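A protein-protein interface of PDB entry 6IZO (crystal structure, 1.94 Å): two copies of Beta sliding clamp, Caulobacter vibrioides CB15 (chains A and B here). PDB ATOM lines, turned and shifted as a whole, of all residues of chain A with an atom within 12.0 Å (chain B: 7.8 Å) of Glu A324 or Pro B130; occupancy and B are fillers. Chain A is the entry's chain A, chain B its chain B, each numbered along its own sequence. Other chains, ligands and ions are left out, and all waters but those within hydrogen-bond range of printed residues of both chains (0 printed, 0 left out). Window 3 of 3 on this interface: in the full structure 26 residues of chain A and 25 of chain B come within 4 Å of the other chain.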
ATOM      1  N   VAL A 296     -26.098  24.725 -17.752  1.00  0.00           N
ATOM      2  CA  VAL A 296     -24.887  24.602 -16.954  1.00  0.00           C
ATOM      3  C   VAL A 296     -23.910  23.580 -17.509  1.00  0.00           C
ATOM      4  O   VAL A 296     -22.695  23.733 -17.350  1.00  0.00           O
ATOM      5  CB  VAL A 296     -25.155  24.369 -15.456  1.00  0.00           C
ATOM      6  CG1 VAL A 296     -25.876  25.583 -14.881  1.00  0.00           C
ATOM      7  CG2 VAL A 296     -25.902  23.064 -15.197  1.00  0.00           C
ATOM      8  N   ALA A 297     -24.425  22.555 -18.177  1.00  0.00           N
ATOM      9  CA  ALA A 297     -23.567  21.520 -18.746  1.00  0.00           C
ATOM     10  C   ALA A 297     -22.742  22.015 -19.950  1.00  0.00           C
ATOM     11  O   ALA A 297     -21.753  21.385 -20.319  1.00  0.00           O
ATOM     12  CB  ALA A 297     -24.393  20.301 -19.127  1.00  0.00           C
ATOM     13  N   THR A 298     -23.160  23.130 -20.552  1.00  0.00           N
ATOM     14  CA  THR A 298     -22.441  23.766 -21.662  1.00  0.00           C
ATOM     15  C   THR A 298     -20.949  23.998 -21.413  1.00  0.00           C
ATOM     16  O   THR A 298     -20.135  23.760 -22.307  1.00  0.00           O
ATOM     17  CB  THR A 298     -23.069  25.120 -22.043  1.00  0.00           C
ATOM     18  OG1 THR A 298     -24.481  24.969 -22.214  1.00  0.00           O
ATOM     19  CG2 THR A 298     -22.484  25.643 -23.359  1.00  0.00           C
ATOM     20  N   ILE A 299     -20.576  24.427 -20.210  1.00  0.00           N
ATOM     21  CA  ILE A 299     -19.181  24.832 -19.973  1.00  0.00           C
ATOM     22  C   ILE A 299     -18.183  23.700 -20.143  1.00  0.00           C
ATOM     23  O   ILE A 299     -16.975  23.953 -20.187  1.00  0.00           O
ATOM     24  CB  ILE A 299     -18.939  25.493 -18.596  1.00  0.00           C
ATOM     25  CG1 ILE A 299     -19.299  24.542 -17.452  1.00  0.00           C
ATOM     26  CG2 ILE A 299     -19.682  26.814 -18.511  1.00  0.00           C
ATOM     27  CD1 ILE A 299     -18.244  24.519 -16.367  1.00  0.00           C
ATOM     28  N   SER A 300     -18.683  22.467 -20.228  1.00  0.00           N
ATOM     29  CA  SER A 300     -17.838  21.293 -20.349  1.00  0.00           C
ATOM     30  C   SER A 300     -17.990  20.494 -21.644  1.00  0.00           C
ATOM     31  O   SER A 300     -18.961  20.639 -22.399  1.00  0.00           O
ATOM     32  CB  SER A 300     -18.117  20.359 -19.182  1.00  0.00           C
ATOM     33  OG  SER A 300     -17.318  19.191 -19.273  1.00  0.00           O
ATOM     34  N   ALA A 301     -16.996  19.626 -21.845  1.00  0.00           N
ATOM     35  CA  ALA A 301     -16.930  18.683 -22.961  1.00  0.00           C
ATOM     36  C   ALA A 301     -16.179  17.413 -22.551  1.00  0.00           C
ATOM     37  O   ALA A 301     -16.224  16.984 -21.396  1.00  0.00           O
ATOM     38  CB  ALA A 301     -16.249  19.326 -24.157  1.00  0.00           C
ATOM     39  N   ARG A 305     -19.774  14.533 -18.477  1.00  0.00           N
ATOM     40  CA  ARG A 305     -19.805  15.673 -17.553  1.00  0.00           C
ATOM     41  C   ARG A 305     -20.764  15.491 -16.382  1.00  0.00           C
ATOM     42  O   ARG A 305     -21.940  15.230 -16.592  1.00  0.00           O
ATOM     43  CB  ARG A 305     -20.193  16.953 -18.302  1.00  0.00           C
ATOM     44  N   VAL A 320     -21.876  23.028 -12.496  1.00  0.00           N
ATOM     45  CA  VAL A 320     -20.927  22.266 -13.309  1.00  0.00           C
ATOM     46  C   VAL A 320     -19.597  23.024 -13.276  1.00  0.00           C
ATOM     47  O   VAL A 320     -19.575  24.264 -13.313  1.00  0.00           O
ATOM     48  CB  VAL A 320     -21.425  22.090 -14.755  1.00  0.00           C
ATOM     49  CG1 VAL A 320     -20.423  21.314 -15.603  1.00  0.00           C
ATOM     50  CG2 VAL A 320     -22.772  21.385 -14.778  1.00  0.00           C
ATOM     51  N   ARG A 321     -18.504  22.273 -13.169  1.00  0.00           N
ATOM     52  CA  ARG A 321     -17.137  22.808 -13.278  1.00  0.00           C
ATOM     53  C   ARG A 321     -16.379  21.990 -14.330  1.00  0.00           C
ATOM     54  O   ARG A 321     -16.783  20.871 -14.648  1.00  0.00           O
ATOM     55  CB  ARG A 321     -16.422  22.752 -11.924  1.00  0.00           C
ATOM     56  N   ASN A 322     -15.316  22.556 -14.900  1.00  0.00           N
ATOM     57  CA  ASN A 322     -14.480  21.826 -15.879  1.00  0.00           C
ATOM     58  C   ASN A 322     -13.010  21.860 -15.488  1.00  0.00           C
ATOM     59  O   ASN A 322     -12.636  22.539 -14.532  1.00  0.00           O
ATOM     60  CB  ASN A 322     -14.708  22.325 -17.327  1.00  0.00           C
ATOM     61  CG  ASN A 322     -14.253  23.769 -17.567  1.00  0.00           C
ATOM     62  OD1 ASN A 322     -13.311  24.248 -16.963  1.00  0.00           O
ATOM     63  ND2 ASN A 322     -14.913  24.451 -18.497  1.00  0.00           N
ATOM     64  N   MET A 323     -12.147  21.200 -16.223  1.00  0.00           N
ATOM     65  CA  MET A 323     -10.766  21.268 -15.827  1.00  0.00           C
ATOM     66  C   MET A 323     -10.160  22.633 -16.126  1.00  0.00           C
ATOM     67  O   MET A 323      -9.232  23.072 -15.452  1.00  0.00           O
ATOM     68  CB  MET A 323      -9.969  20.151 -16.474  1.00  0.00           C
ATOM     69  N   GLU A 324     -10.688  23.308 -17.125  1.00  0.00           N
ATOM     70  CA  GLU A 324     -10.165  24.599 -17.511  1.00  0.00           C
ATOM     71  C   GLU A 324     -10.619  25.787 -16.700  1.00  0.00           C
ATOM     72  O   GLU A 324     -10.614  26.876 -17.190  1.00  0.00           O
ATOM     73  CB  GLU A 324     -10.472  24.863 -18.982  1.00  0.00           C
ATOM     74  N   ALA A 325     -11.010  25.597 -15.467  1.00  0.00           N
ATOM     75  CA  ALA A 325     -11.460  26.721 -14.604  1.00  0.00           C
ATOM     76  C   ALA A 325     -12.879  27.331 -14.732  1.00  0.00           C
ATOM     77  O   ALA A 325     -13.310  28.098 -13.910  1.00  0.00           O
ATOM     78  CB  ALA A 325     -10.435  27.816 -14.620  1.00  0.00           C
ATOM     79  N   GLY A 326     -13.553  26.973 -15.794  1.00  0.00           N
ATOM     80  CA  GLY A 326     -14.939  27.248 -16.166  1.00  0.00           C
ATOM     81  C   GLY A 326     -15.911  26.761 -15.106  1.00  0.00           C
ATOM     82  O   GLY A 326     -15.750  25.658 -14.585  1.00  0.00           O
ATOM     83  N   GLN A 327     -16.910  27.589 -14.793  1.00  0.00           N
ATOM     84  CA  GLN A 327     -17.961  27.242 -13.838  1.00  0.00           C
ATOM     85  C   GLN A 327     -19.298  27.777 -14.325  1.00  0.00           C
ATOM     86  O   GLN A 327     -19.358  28.839 -14.931  1.00  0.00           O
ATOM     87  CB  GLN A 327     -17.644  27.815 -12.465  1.00  0.00           C
ATOM     88  CG  GLN A 327     -18.614  27.410 -11.369  1.00  0.00           C
ATOM     89  CD  GLN A 327     -18.269  28.065 -10.050  1.00  0.00           C
ATOM     90  OE1 GLN A 327     -18.521  29.255  -9.862  1.00  0.00           O
ATOM     91  NE2 GLN A 327     -17.698  27.297  -9.129  1.00  0.00           N
ATOM     92  N   ALA A 328     -20.359  27.019 -14.059  1.00  0.00           N
ATOM     93  CA  ALA A 328     -21.731  27.397 -14.405  1.00  0.00           C
ATOM     94  C   ALA A 328     -22.608  27.047 -13.207  1.00  0.00           C
ATOM     95  O   ALA A 328     -22.457  25.965 -12.629  1.00  0.00           O
ATOM     96  CB  ALA A 328     -22.203  26.652 -15.645  1.00  0.00           C
ATOM     97  N   ASN B  52     -10.605  31.764 -28.959  1.00  0.00           N
ATOM     98  CA  ASN B  52     -11.316  32.853 -28.278  1.00  0.00           C
ATOM     99  C   ASN B  52     -11.847  33.946 -29.193  1.00  0.00           C
ATOM    100  O   ASN B  52     -11.335  34.170 -30.285  1.00  0.00           O
ATOM    101  CB  ASN B  52     -10.411  33.464 -27.203  1.00  0.00           C
ATOM    102  CG  ASN B  52     -10.187  32.526 -26.030  1.00  0.00           C
ATOM    103  OD1 ASN B  52     -10.643  31.382 -26.044  1.00  0.00           O
ATOM    104  ND2 ASN B  52      -9.513  33.022 -24.986  1.00  0.00           N
ATOM    105  N   ILE B  87     -11.178  42.027 -23.543  1.00  0.00           N
ATOM    106  CA  ILE B  87     -10.760  40.707 -23.006  1.00  0.00           C
ATOM    107  C   ILE B  87     -11.015  39.649 -24.067  1.00  0.00           C
ATOM    108  O   ILE B  87     -11.756  39.914 -25.023  1.00  0.00           O
ATOM    109  CB  ILE B  87     -11.531  40.318 -21.715  1.00  0.00           C
ATOM    110  CG1 ILE B  87     -13.056  40.433 -21.882  1.00  0.00           C
ATOM    111  CG2 ILE B  87     -11.091  41.173 -20.542  1.00  0.00           C
ATOM    112  CD1 ILE B  87     -13.771  39.124 -22.112  1.00  0.00           C
ATOM    113  N   THR B  88     -10.409  38.474 -23.928  1.00  0.00           N
ATOM    114  CA  THR B  88     -10.750  37.355 -24.841  1.00  0.00           C
ATOM    115  C   THR B  88     -11.351  36.219 -24.041  1.00  0.00           C
ATOM    116  O   THR B  88     -10.979  36.033 -22.884  1.00  0.00           O
ATOM    117  CB  THR B  88      -9.571  36.839 -25.676  1.00  0.00           C
ATOM    118  OG1 THR B  88      -8.760  35.982 -24.883  1.00  0.00           O
ATOM    119  CG2 THR B  88      -8.716  37.996 -26.209  1.00  0.00           C
ATOM    120  N   ALA B  89     -12.274  35.480 -24.662  1.00  0.00           N
ATOM    121  CA  ALA B  89     -12.997  34.406 -23.998  1.00  0.00           C
ATOM    122  C   ALA B  89     -13.395  33.321 -25.024  1.00  0.00           C
ATOM    123  O   ALA B  89     -13.507  33.615 -26.211  1.00  0.00           O
ATOM    124  CB  ALA B  89     -14.226  34.960 -23.294  1.00  0.00           C
ATOM    125  N   PRO B  90     -13.600  32.067 -24.571  1.00  0.00           N
ATOM    126  CA  PRO B  90     -13.835  30.943 -25.488  1.00  0.00           C
ATOM    127  C   PRO B  90     -15.070  31.131 -26.381  1.00  0.00           C
ATOM    128  O   PRO B  90     -16.176  31.338 -25.872  1.00  0.00           O
ATOM    129  CB  PRO B  90     -13.984  29.740 -24.545  1.00  0.00           C
ATOM    130  CG  PRO B  90     -13.199  30.122 -23.340  1.00  0.00           C
ATOM    131  CD  PRO B  90     -13.458  31.598 -23.178  1.00  0.00           C
ATOM    132  N   THR B  93     -18.058  28.114 -26.644  1.00  0.00           N
ATOM    133  CA  THR B  93     -18.713  28.038 -25.331  1.00  0.00           C
ATOM    134  C   THR B  93     -19.561  29.275 -25.062  1.00  0.00           C
ATOM    135  O   THR B  93     -20.728  29.171 -24.611  1.00  0.00           O
ATOM    136  CB  THR B  93     -17.671  27.827 -24.222  1.00  0.00           C
ATOM    137  OG1 THR B  93     -16.937  26.634 -24.514  1.00  0.00           O
ATOM    138  CG2 THR B  93     -18.312  27.718 -22.839  1.00  0.00           C
ATOM    139  N   PHE B 111     -16.429  41.510 -14.829  1.00  0.00           N
ATOM    140  CA  PHE B 111     -15.515  40.915 -13.844  1.00  0.00           C
ATOM    141  C   PHE B 111     -15.922  41.283 -12.424  1.00  0.00           C
ATOM    142  O   PHE B 111     -15.523  40.614 -11.482  1.00  0.00           O
ATOM    143  CB  PHE B 111     -14.084  41.372 -14.114  1.00  0.00           C
ATOM    144  CG  PHE B 111     -13.539  40.794 -15.365  1.00  0.00           C
ATOM    145  CD1 PHE B 111     -12.745  39.648 -15.333  1.00  0.00           C
ATOM    146  CD2 PHE B 111     -13.878  41.345 -16.591  1.00  0.00           C
ATOM    147  CE1 PHE B 111     -12.263  39.087 -16.504  1.00  0.00           C
ATOM    148  CE2 PHE B 111     -13.407  40.798 -17.761  1.00  0.00           C
ATOM    149  CZ  PHE B 111     -12.603  39.653 -17.720  1.00  0.00           C
ATOM    150  N   PRO B 116     -10.638  36.249 -11.722  1.00  0.00           N
ATOM    151  CA  PRO B 116     -10.061  36.705 -12.967  1.00  0.00           C
ATOM    152  C   PRO B 116     -10.794  36.151 -14.214  1.00  0.00           C
ATOM    153  O   PRO B 116     -10.243  36.206 -15.287  1.00  0.00           O
ATOM    154  CB  PRO B 116      -8.661  36.131 -12.882  1.00  0.00           C
ATOM    155  CG  PRO B 116      -8.886  34.789 -12.288  1.00  0.00           C
ATOM    156  CD  PRO B 116     -10.026  34.966 -11.313  1.00  0.00           C
ATOM    157  N   ARG B 117     -12.020  35.645 -14.061  1.00  0.00           N
ATOM    158  CA  ARG B 117     -12.784  35.043 -15.161  1.00  0.00           C
ATOM    159  C   ARG B 117     -13.872  36.002 -15.642  1.00  0.00           C
ATOM    160  O   ARG B 117     -14.325  36.867 -14.894  1.00  0.00           O
ATOM    161  CB  ARG B 117     -13.384  33.710 -14.687  1.00  0.00           C
ATOM    162  CG  ARG B 117     -12.326  32.634 -14.440  1.00  0.00           C
ATOM    163  CD  ARG B 117     -12.876  31.392 -13.749  1.00  0.00           C
ATOM    164  NE  ARG B 117     -13.485  31.719 -12.463  1.00  0.00           N
ATOM    165  CZ  ARG B 117     -13.977  30.849 -11.580  1.00  0.00           C
ATOM    166  NH1 ARG B 117     -13.962  29.542 -11.809  1.00  0.00           N
ATOM    167  NH2 ARG B 117     -14.509  31.313 -10.455  1.00  0.00           N
ATOM    168  N   LEU B 118     -14.283  35.860 -16.903  1.00  0.00           N
ATOM    169  CA  LEU B 118     -15.417  36.616 -17.441  1.00  0.00           C
ATOM    170  C   LEU B 118     -16.677  36.066 -16.802  1.00  0.00           C
ATOM    171  O   LEU B 118     -16.919  34.857 -16.888  1.00  0.00           O
ATOM    172  CB  LEU B 118     -15.534  36.430 -18.936  1.00  0.00           C
ATOM    173  CG  LEU B 118     -16.764  36.985 -19.663  1.00  0.00           C
ATOM    174  CD1 LEU B 118     -16.883  38.498 -19.553  1.00  0.00           C
ATOM    175  CD2 LEU B 118     -16.750  36.559 -21.116  1.00  0.00           C
ATOM    176  N   VAL B 119     -17.483  36.948 -16.215  1.00  0.00           N
ATOM    177  CA  VAL B 119     -18.736  36.570 -15.573  1.00  0.00           C
ATOM    178  C   VAL B 119     -19.869  36.915 -16.545  1.00  0.00           C
ATOM    179  O   VAL B 119     -19.996  38.068 -16.959  1.00  0.00           O
ATOM    180  CB  VAL B 119     -18.958  37.324 -14.236  1.00  0.00           C
ATOM    181  CG1 VAL B 119     -20.259  36.888 -13.556  1.00  0.00           C
ATOM    182  CG2 VAL B 119     -17.782  37.126 -13.297  1.00  0.00           C
ATOM    183  N   ILE B 120     -20.657  35.901 -16.920  1.00  0.00           N
ATOM    184  CA  ILE B 120     -21.846  36.058 -17.736  1.00  0.00           C
ATOM    185  C   ILE B 120     -23.023  35.746 -16.842  1.00  0.00           C
ATOM    186  O   ILE B 120     -23.112  34.645 -16.299  1.00  0.00           O
ATOM    187  CB  ILE B 120     -21.872  35.095 -18.946  1.00  0.00           C
ATOM    188  CG1 ILE B 120     -20.618  35.289 -19.817  1.00  0.00           C
ATOM    189  CG2 ILE B 120     -23.127  35.309 -19.782  1.00  0.00           C
ATOM    190  CD1 ILE B 120     -19.590  34.204 -19.688  1.00  0.00           C
ATOM    191  N   PHE B 127     -22.231  32.274 -15.206  1.00  0.00           N
ATOM    192  CA  PHE B 127     -21.115  31.531 -15.785  1.00  0.00           C
ATOM    193  C   PHE B 127     -19.818  32.304 -15.590  1.00  0.00           C
ATOM    194  O   PHE B 127     -19.799  33.532 -15.700  1.00  0.00           O
ATOM    195  CB  PHE B 127     -21.316  31.282 -17.275  1.00  0.00           C
ATOM    196  CG  PHE B 127     -22.597  30.604 -17.620  1.00  0.00           C
ATOM    197  CD1 PHE B 127     -23.785  31.316 -17.657  1.00  0.00           C
ATOM    198  CD2 PHE B 127     -22.614  29.251 -17.939  1.00  0.00           C
ATOM    199  CE1 PHE B 127     -24.972  30.691 -17.979  1.00  0.00           C
ATOM    200  CE2 PHE B 127     -23.800  28.623 -18.265  1.00  0.00           C
ATOM    201  CZ  PHE B 127     -24.978  29.344 -18.294  1.00  0.00           C
ATOM    202  N   ASN B 128     -18.750  31.568 -15.312  1.00  0.00           N
ATOM    203  CA  ASN B 128     -17.402  32.113 -15.186  1.00  0.00           C
ATOM    204  C   ASN B 128     -16.549  31.365 -16.201  1.00  0.00           C
ATOM    205  O   ASN B 128     -16.383  30.157 -16.092  1.00  0.00           O
ATOM    206  CB  ASN B 128     -16.839  31.916 -13.777  1.00  0.00           C
ATOM    207  CG  ASN B 128     -17.818  32.331 -12.689  1.00  0.00           C
ATOM    208  OD1 ASN B 128     -17.790  33.459 -12.189  1.00  0.00           O
ATOM    209  ND2 ASN B 128     -18.694  31.418 -12.322  1.00  0.00           N
ATOM    210  N   LEU B 129     -16.056  32.070 -17.212  1.00  0.00           N
ATOM    211  CA  LEU B 129     -15.195  31.487 -18.232  1.00  0.00           C
ATOM    212  C   LEU B 129     -13.775  31.996 -18.094  1.00  0.00           C
ATOM    213  O   LEU B 129     -13.574  33.171 -17.815  1.00  0.00           O
ATOM    214  CB  LEU B 129     -15.700  31.853 -19.631  1.00  0.00           C
ATOM    215  CG  LEU B 129     -17.108  31.418 -20.025  1.00  0.00           C
ATOM    216  CD1 LEU B 129     -17.375  31.827 -21.469  1.00  0.00           C
ATOM    217  CD2 LEU B 129     -17.298  29.918 -19.839  1.00  0.00           C
ATOM    218  N   PRO B 130     -12.780  31.121 -18.312  1.00  0.00           N
ATOM    219  CA  PRO B 130     -11.403  31.614 -18.299  1.00  0.00           C
ATOM    220  C   PRO B 130     -11.144  32.556 -19.465  1.00  0.00           C
ATOM    221  O   PRO B 130     -11.751  32.399 -20.532  1.00  0.00           O
ATOM    222  CB  PRO B 130     -10.550  30.350 -18.431  1.00  0.00           C
ATOM    223  CG  PRO B 130     -11.458  29.308 -18.999  1.00  0.00           C
ATOM    224  CD  PRO B 130     -12.850  29.664 -18.541  1.00  0.00           C
ATOM    225  N   VAL B 131     -10.254  33.519 -19.235  1.00  0.00           N
ATOM    226  CA  VAL B 131      -9.921  34.538 -20.224  1.00  0.00           C
ATOM    227  C   VAL B 131      -8.438  34.529 -20.555  1.00  0.00           C
ATOM    228  O   VAL B 131      -7.601  33.981 -19.821  1.00  0.00           O
ATOM    229  CB  VAL B 131     -10.332  35.955 -19.770  1.00  0.00           C
ATOM    230  CG1 VAL B 131     -11.823  36.013 -19.521  1.00  0.00           C
ATOM    231  CG2 VAL B 131      -9.568  36.408 -18.521  1.00  0.00           C
ATOM    232  N   LEU B 132      -8.123  35.142 -21.689  1.00  0.00           N
ATOM    233  CA  LEU B 132      -6.737  35.336 -22.078  1.00  0.00           C
ATOM    234  C   LEU B 132      -6.586  36.793 -22.434  1.00  0.00           C
ATOM    235  O   LEU B 132      -7.553  37.443 -22.883  1.00  0.00           O
ATOM    236  CB  LEU B 132      -6.280  34.385 -23.185  1.00  0.00           C
ATOM    237  CG  LEU B 132      -6.095  32.923 -22.743  1.00  0.00           C
ATOM    238  CD1 LEU B 132      -6.046  31.959 -23.920  1.00  0.00           C
ATOM    239  CD2 LEU B 132      -4.859  32.712 -21.856  1.00  0.00           C
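The guanidinium group of Arg B117 is in hydrogen-bond range of the backbone carbonyl oxygen of Ala A325. O of Gln A327 is in hydrogen-bond range of N of Asn B128, 2.8 Å away.
Among the printed residues, merely in contact across the chains: Ile A299 with Phe B127 (3.9 Å), Glu A324 with Pro B130 (3.1 Å), Gly A326 with Asn B128 (3.2 Å), Gly A326 with Pro B130 (3.9 Å), Gln A327 with Phe B127 (3.3 Å) and Ala A328 with Phe B127 (3.5 Å).
The backbone NH (N) of Ala A325 sits at hydrogen-bond distance from the side-chain amide oxygen (OD1) of Asn A322, at 3.1 Å. The backbone carbonyl oxygen of Val A320 sits at hydrogen-bond distance from the backbone NH of Ala A328 (3.0 Å). The side-chain amide oxygen (OD1) of Asn A322 sits at hydrogen-bond distance from the backbone NH (N) of Glu A324, 2.8 Å away. The backbone carbonyl oxygen (O) of Ile B120 sits at hydrogen-bond distance from the backbone NH (N) of Phe B127 (2.8 Å). O of Ile A299 sits at hydrogen-bond distance from ND2 of Asn A322 (2.7 Å). N of Gly A326 sits at hydrogen-bond distance from OD1 of Asn A322.
Of the 16 printed residues of chain A, 6 touch a printed residue of chain B. Hydrophobic or aromatic side chains of chain A within 4 Å of the printed part of chain B: Ile A299 and Ala A328. Hydrophobic or aromatic side chains of chain B within 4 Å of the printed part of chain A: Phe B127 and Pro B130. Among the printed residues, 8 pairs touch across the chains.
No position is printed for both chains. Of the 8 pairs that touch across the chains among the printed residues, none has its exchanged pair printed and touching as well.
Thr A298 touches none of the printed residues of chain B. No residue of chain B comes within 4 Å of Met A323. Of chain B, only Pro B130 comes within 4 Å of Glu A324. Of the printed residues of chain B, Ala A328 touches Phe B127. Of the printed residues of chain A, Asn B128 touches Gly A326 and Gln A327. Leu B129 touches none of the printed residues of chain A. Printed residues of chain A within 4 Å of Pro B130: Glu A324 (3.1 Å) and Gly A326 (3.9 Å). No residue of chain A comes within 4 Å of Val B131.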
